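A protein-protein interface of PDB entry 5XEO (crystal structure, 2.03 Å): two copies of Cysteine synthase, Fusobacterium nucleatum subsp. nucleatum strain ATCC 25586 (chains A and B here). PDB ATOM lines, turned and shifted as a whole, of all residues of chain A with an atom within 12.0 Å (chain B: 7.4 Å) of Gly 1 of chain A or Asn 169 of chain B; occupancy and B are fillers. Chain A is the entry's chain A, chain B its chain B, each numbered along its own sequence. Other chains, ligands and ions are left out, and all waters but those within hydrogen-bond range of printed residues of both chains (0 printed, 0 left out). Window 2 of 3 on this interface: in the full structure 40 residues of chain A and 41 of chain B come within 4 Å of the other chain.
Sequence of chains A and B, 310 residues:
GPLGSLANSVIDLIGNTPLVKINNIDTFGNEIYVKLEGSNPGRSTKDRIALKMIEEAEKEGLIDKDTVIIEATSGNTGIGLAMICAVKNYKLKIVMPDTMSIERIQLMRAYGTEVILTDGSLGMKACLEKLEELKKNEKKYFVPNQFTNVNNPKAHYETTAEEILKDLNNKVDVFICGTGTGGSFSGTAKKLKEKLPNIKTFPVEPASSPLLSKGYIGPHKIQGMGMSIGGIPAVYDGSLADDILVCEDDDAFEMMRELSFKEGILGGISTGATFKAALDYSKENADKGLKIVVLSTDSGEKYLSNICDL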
ATOM      1  N   GLY A   1     -20.451  26.826 -17.634  1.00  0.00           N
ATOM      2  CA  GLY A   1     -21.286  27.869 -18.292  1.00  0.00           C
ATOM      3  C   GLY A   1     -21.386  27.680 -19.807  1.00  0.00           C
ATOM      4  O   GLY A   1     -20.647  26.849 -20.376  1.00  0.00           O
ATOM      5  N   PRO A   2     -22.268  28.472 -20.474  1.00  0.00           N
ATOM      6  CA  PRO A   2     -22.637  28.331 -21.909  1.00  0.00           C
ATOM      7  C   PRO A   2     -21.479  28.404 -22.912  1.00  0.00           C
ATOM      8  O   PRO A   2     -21.512  27.712 -23.932  1.00  0.00           O
ATOM      9  CB  PRO A   2     -23.626  29.492 -22.143  1.00  0.00           C
ATOM     10  CG  PRO A   2     -23.330  30.480 -21.066  1.00  0.00           C
ATOM     11  CD  PRO A   2     -22.878  29.679 -19.878  1.00  0.00           C
ATOM     12  N   LEU A   3     -20.470  29.226 -22.620  1.00  0.00           N
ATOM     13  CA  LEU A   3     -19.271  29.329 -23.471  1.00  0.00           C
ATOM     14  C   LEU A   3     -18.066  28.569 -22.858  1.00  0.00           C
ATOM     15  O   LEU A   3     -16.920  28.851 -23.194  1.00  0.00           O
ATOM     16  CB  LEU A   3     -18.932  30.809 -23.807  1.00  0.00           C
ATOM     17  CG  LEU A   3     -19.247  31.969 -22.842  1.00  0.00           C
ATOM     18  CD1 LEU A   3     -18.323  33.158 -23.095  1.00  0.00           C
ATOM     19  CD2 LEU A   3     -20.712  32.404 -22.934  1.00  0.00           C
ATOM     20  N   GLY A   4     -18.338  27.581 -22.000  1.00  0.00           N
ATOM     21  CA  GLY A   4     -17.288  26.767 -21.385  1.00  0.00           C
ATOM     22  C   GLY A   4     -16.880  25.611 -22.284  1.00  0.00           C
ATOM     23  O   GLY A   4     -17.475  25.388 -23.340  1.00  0.00           O
ATOM     24  N   SER A   5     -15.838  24.895 -21.869  1.00  0.00           N
ATOM     25  CA  SER A   5     -15.371  23.713 -22.562  1.00  0.00           C
ATOM     26  C   SER A   5     -15.393  22.429 -21.680  1.00  0.00           C
ATOM     27  O   SER A   5     -14.461  21.617 -21.765  1.00  0.00           O
ATOM     28  CB  SER A   5     -13.963  24.002 -23.110  1.00  0.00           C
ATOM     29  OG  SER A   5     -13.979  25.124 -23.981  1.00  0.00           O
ATOM     30  N   LEU A   6     -16.447  22.224 -20.865  1.00  0.00           N
ATOM     31  CA  LEU A   6     -16.684  20.889 -20.259  1.00  0.00           C
ATOM     32  C   LEU A   6     -17.046  19.850 -21.347  1.00  0.00           C
ATOM     33  O   LEU A   6     -17.902  20.134 -22.185  1.00  0.00           O
ATOM     34  CB  LEU A   6     -17.788  20.911 -19.204  1.00  0.00           C
ATOM     35  CG  LEU A   6     -17.651  19.828 -18.136  1.00  0.00           C
ATOM     36  CD1 LEU A   6     -16.519  20.191 -17.186  1.00  0.00           C
ATOM     37  CD2 LEU A   6     -18.911  19.626 -17.331  1.00  0.00           C
ATOM     38  N   ALA A   7     -16.413  18.670 -21.319  1.00  0.00           N
ATOM     39  CA  ALA A   7     -16.636  17.605 -22.325  1.00  0.00           C
ATOM     40  C   ALA A   7     -16.936  16.282 -21.635  1.00  0.00           C
ATOM     41  O   ALA A   7     -16.265  15.947 -20.655  1.00  0.00           O
ATOM     42  CB  ALA A   7     -15.406  17.435 -23.202  1.00  0.00           C
ATOM     43  N   ASN A   8     -17.885  15.507 -22.165  1.00  0.00           N
ATOM     44  CA  ASN A   8     -18.188  14.164 -21.610  1.00  0.00           C
ATOM     45  C   ASN A   8     -17.113  13.161 -21.916  1.00  0.00           C
ATOM     46  O   ASN A   8     -16.890  12.239 -21.133  1.00  0.00           O
ATOM     47  CB  ASN A   8     -19.479  13.599 -22.154  1.00  0.00           C
ATOM     48  CG  ASN A   8     -20.655  14.460 -21.808  1.00  0.00           C
ATOM     49  OD1 ASN A   8     -20.937  14.678 -20.629  1.00  0.00           O
ATOM     50  ND2 ASN A   8     -21.337  14.974 -22.828  1.00  0.00           N
ATOM     51  N   GLU B 163     -10.916  29.188 -15.851  1.00  0.00           N
ATOM     52  CA  GLU B 163     -11.510  28.203 -16.754  1.00  0.00           C
ATOM     53  C   GLU B 163     -12.090  26.987 -16.025  1.00  0.00           C
ATOM     54  O   GLU B 163     -13.152  26.512 -16.408  1.00  0.00           O
ATOM     55  CB  GLU B 163     -10.501  27.741 -17.796  1.00  0.00           C
ATOM     56  CG  GLU B 163     -10.043  28.862 -18.713  1.00  0.00           C
ATOM     57  CD  GLU B 163      -8.878  28.448 -19.585  1.00  0.00           C
ATOM     58  OE1 GLU B 163      -8.624  27.221 -19.785  1.00  0.00           O
ATOM     59  OE2 GLU B 163      -8.201  29.348 -20.100  1.00  0.00           O
ATOM     60  N   ILE B 164     -11.416  26.528 -14.977  1.00  0.00           N
ATOM     61  CA  ILE B 164     -11.869  25.399 -14.160  1.00  0.00           C
ATOM     62  C   ILE B 164     -13.151  25.817 -13.455  1.00  0.00           C
ATOM     63  O   ILE B 164     -14.167  25.085 -13.494  1.00  0.00           O
ATOM     64  CB  ILE B 164     -10.766  24.909 -13.187  1.00  0.00           C
ATOM     65  CG1 ILE B 164      -9.633  24.209 -13.982  1.00  0.00           C
ATOM     66  CG2 ILE B 164     -11.336  24.013 -12.101  1.00  0.00           C
ATOM     67  CD1 ILE B 164      -8.300  24.073 -13.254  1.00  0.00           C
ATOM     68  N   LEU B 165     -13.124  26.983 -12.818  1.00  0.00           N
ATOM     69  CA  LEU B 165     -14.319  27.469 -12.091  1.00  0.00           C
ATOM     70  C   LEU B 165     -15.563  27.614 -12.994  1.00  0.00           C
ATOM     71  O   LEU B 165     -16.690  27.250 -12.595  1.00  0.00           O
ATOM     72  CB  LEU B 165     -14.022  28.788 -11.399  1.00  0.00           C
ATOM     73  CG  LEU B 165     -13.043  28.690 -10.232  1.00  0.00           C
ATOM     74  CD1 LEU B 165     -12.504  30.053  -9.889  1.00  0.00           C
ATOM     75  CD2 LEU B 165     -13.682  28.081  -9.002  1.00  0.00           C
ATOM     76  N   LYS B 166     -15.358  28.146 -14.193  1.00  0.00           N
ATOM     77  CA  LYS B 166     -16.459  28.410 -15.133  1.00  0.00           C
ATOM     78  C   LYS B 166     -17.004  27.128 -15.717  1.00  0.00           C
ATOM     79  O   LYS B 166     -18.221  26.937 -15.713  1.00  0.00           O
ATOM     80  CB  LYS B 166     -16.000  29.332 -16.261  1.00  0.00           C
ATOM     81  CG  LYS B 166     -15.773  30.738 -15.755  1.00  0.00           C
ATOM     82  CD  LYS B 166     -14.960  31.584 -16.736  1.00  0.00           C
ATOM     83  CE  LYS B 166     -15.059  33.058 -16.384  1.00  0.00           C
ATOM     84  NZ  LYS B 166     -14.067  33.857 -17.150  1.00  0.00           N
ATOM     85  N   ASP B 167     -16.105  26.232 -16.157  1.00  0.00           N
ATOM     86  CA  ASP B 167     -16.489  24.974 -16.786  1.00  0.00           C
ATOM     87  C   ASP B 167     -17.274  24.054 -15.802  1.00  0.00           C
ATOM     88  O   ASP B 167     -18.169  23.328 -16.217  1.00  0.00           O
ATOM     89  CB  ASP B 167     -15.256  24.224 -17.356  1.00  0.00           C
ATOM     90  CG  ASP B 167     -14.694  24.864 -18.654  1.00  0.00           C
ATOM     91  OD1 ASP B 167     -15.331  25.833 -19.188  1.00  0.00           O
ATOM     92  OD2 ASP B 167     -13.625  24.386 -19.152  1.00  0.00           O
ATOM     93  N   LEU B 168     -16.890  24.067 -14.529  1.00  0.00           N
ATOM     94  CA  LEU B 168     -17.570  23.279 -13.502  1.00  0.00           C
ATOM     95  C   LEU B 168     -18.604  24.084 -12.688  1.00  0.00           C
ATOM     96  O   LEU B 168     -19.102  23.599 -11.688  1.00  0.00           O
ATOM     97  CB  LEU B 168     -16.554  22.597 -12.595  1.00  0.00           C
ATOM     98  CG  LEU B 168     -15.895  21.373 -13.214  1.00  0.00           C
ATOM     99  CD1 LEU B 168     -14.857  20.819 -12.277  1.00  0.00           C
ATOM    100  CD2 LEU B 168     -16.911  20.285 -13.538  1.00  0.00           C
ATOM    101  N   ASN B 169     -18.903  25.304 -13.131  1.00  0.00           N
ATOM    102  CA  ASN B 169     -19.863  26.188 -12.507  1.00  0.00           C
ATOM    103  C   ASN B 169     -19.618  26.321 -10.994  1.00  0.00           C
ATOM    104  O   ASN B 169     -20.535  26.239 -10.189  1.00  0.00           O
ATOM    105  CB  ASN B 169     -21.287  25.729 -12.890  1.00  0.00           C
ATOM    106  CG  ASN B 169     -21.514  25.726 -14.413  1.00  0.00           C
ATOM    107  OD1 ASN B 169     -21.403  26.765 -15.082  1.00  0.00           O
ATOM    108  ND2 ASN B 169     -21.822  24.549 -14.974  1.00  0.00           N
ATOM    109  N   ASN B 170     -18.354  26.528 -10.620  1.00  0.00           N
ATOM    110  CA  ASN B 170     -17.922  26.676  -9.233  1.00  0.00           C
ATOM    111  C   ASN B 170     -18.046  25.449  -8.330  1.00  0.00           C
ATOM    112  O   ASN B 170     -17.898  25.570  -7.124  1.00  0.00           O
ATOM    113  CB  ASN B 170     -18.572  27.903  -8.568  1.00  0.00           C
ATOM    114  CG  ASN B 170     -18.208  29.178  -9.265  1.00  0.00           C
ATOM    115  OD1 ASN B 170     -17.076  29.342  -9.711  1.00  0.00           O
ATOM    116  ND2 ASN B 170     -19.176  30.076  -9.416  1.00  0.00           N
ATOM    117  N   LYS B 171     -18.252  24.276  -8.916  1.00  0.00           N
ATOM    118  CA  LYS B 171     -18.336  23.046  -8.158  1.00  0.00           C
ATOM    119  C   LYS B 171     -17.045  22.284  -8.366  1.00  0.00           C
ATOM    120  O   LYS B 171     -16.923  21.483  -9.290  1.00  0.00           O
ATOM    121  CB  LYS B 171     -19.526  22.192  -8.619  1.00  0.00           C
ATOM    122  CG  LYS B 171     -20.811  22.928  -8.882  1.00  0.00           C
ATOM    123  CD  LYS B 171     -21.443  23.433  -7.611  1.00  0.00           C
ATOM    124  CE  LYS B 171     -22.793  24.067  -7.927  1.00  0.00           C
ATOM    125  NZ  LYS B 171     -23.687  24.082  -6.738  1.00  0.00           N
ATOM    126  N   VAL B 172     -16.073  22.547  -7.512  1.00  0.00           N
ATOM    127  CA  VAL B 172     -14.800  21.847  -7.565  1.00  0.00           C
ATOM    128  C   VAL B 172     -14.423  21.520  -6.153  1.00  0.00           C
ATOM    129  O   VAL B 172     -14.384  22.414  -5.352  1.00  0.00           O
ATOM    130  CB  VAL B 172     -13.687  22.714  -8.205  1.00  0.00           C
ATOM    131  CG1 VAL B 172     -12.472  21.839  -8.515  1.00  0.00           C
ATOM    132  CG2 VAL B 172     -14.197  23.354  -9.468  1.00  0.00           C
ATOM    133  N   LEU B 196     -13.105  29.254  -3.609  1.00  0.00           N
ATOM    134  CA  LEU B 196     -13.698  28.065  -3.046  1.00  0.00           C
ATOM    135  C   LEU B 196     -12.909  27.744  -1.799  1.00  0.00           C
ATOM    136  O   LEU B 196     -11.960  26.980  -1.848  1.00  0.00           O
ATOM    137  CB  LEU B 196     -13.682  26.915  -4.071  1.00  0.00           C
ATOM    138  CG  LEU B 196     -14.503  27.160  -5.348  1.00  0.00           C
ATOM    139  CD1 LEU B 196     -14.287  26.044  -6.368  1.00  0.00           C
ATOM    140  CD2 LEU B 196     -15.978  27.286  -5.058  1.00  0.00           C
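Among the printed residues, merely in contact across the chains: Gly 4 of chain A with Asp 167 of chain B, Leu 6 of chain A with Asp 167 of chain B and Leu 6 of chain A with Leu 168 of chain B.
Hydrophobic or aromatic side chains of chain B that line the printed part of chain A: Leu 168.
Of the 8 printed residues of chain A, 4 touch a printed residue of chain B.
Hydrophobic or aromatic side chains of chain A that line the printed part of chain B: Leu 6.
Among the printed residues, 6 pairs touch across the chains.
Among the printed residues, no Asp or Glu carboxylate lies within 4 Å of a Lys or Arg side-chain nitrogen of the other chain.
O of Lys 166 of chain B lies close to OD1 of Asn 169 of chain B.
OD1 of Asn 169 of chain B lies within hydrogen-bond range of N of Gly 1 of chain A, 2.7 Å away.
OD1 of Asp 167 of chain B lies within hydrogen-bond range of N of Ser 5 of chain A, at 2.9 Å.
The backbone NH (N) of Gly 1 of chain A sits at hydrogen-bond distance from the backbone carbonyl oxygen (O) of Lys 166 of chain B (2.9 Å).
No position is printed for both chains.
Of the 6 pairs that touch across the chains among the printed residues, none has its exchanged pair printed and touching as well.
Printed residues of chain B within 4 Å of Gly 1 of chain A: Lys 166 (2.9 Å) and Asn 169 (2.7 Å).
Asp 167 of chain B touches just these residues of chain A: Gly 4 (3.1 Å), Ser 5 (2.9 Å) and Leu 6 (3.7 Å).
Of chain A, only Leu 6 comes within 4 Å of Leu 168 of chain B.
Printed residues of chain A within 4 Å of Lys 166 of chain B: Gly 1 (2.9 Å).
Of the printed residues of chain B, Leu 6 of chain A touches Asp 167 and Leu 168.
Leu 3 of chain A touches none of the printed residues of chain B.
Leu 165 of chain B touches none of the printed residues of chain A.
The nearest residue of chain B that does not touch Gly 1 of chain A is Asp 167 of chain B (4.4 Å).
The nearest printed residue of chain B that does not touch Gly 4 of chain A is Lys 166 of chain B (5.7 Å).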
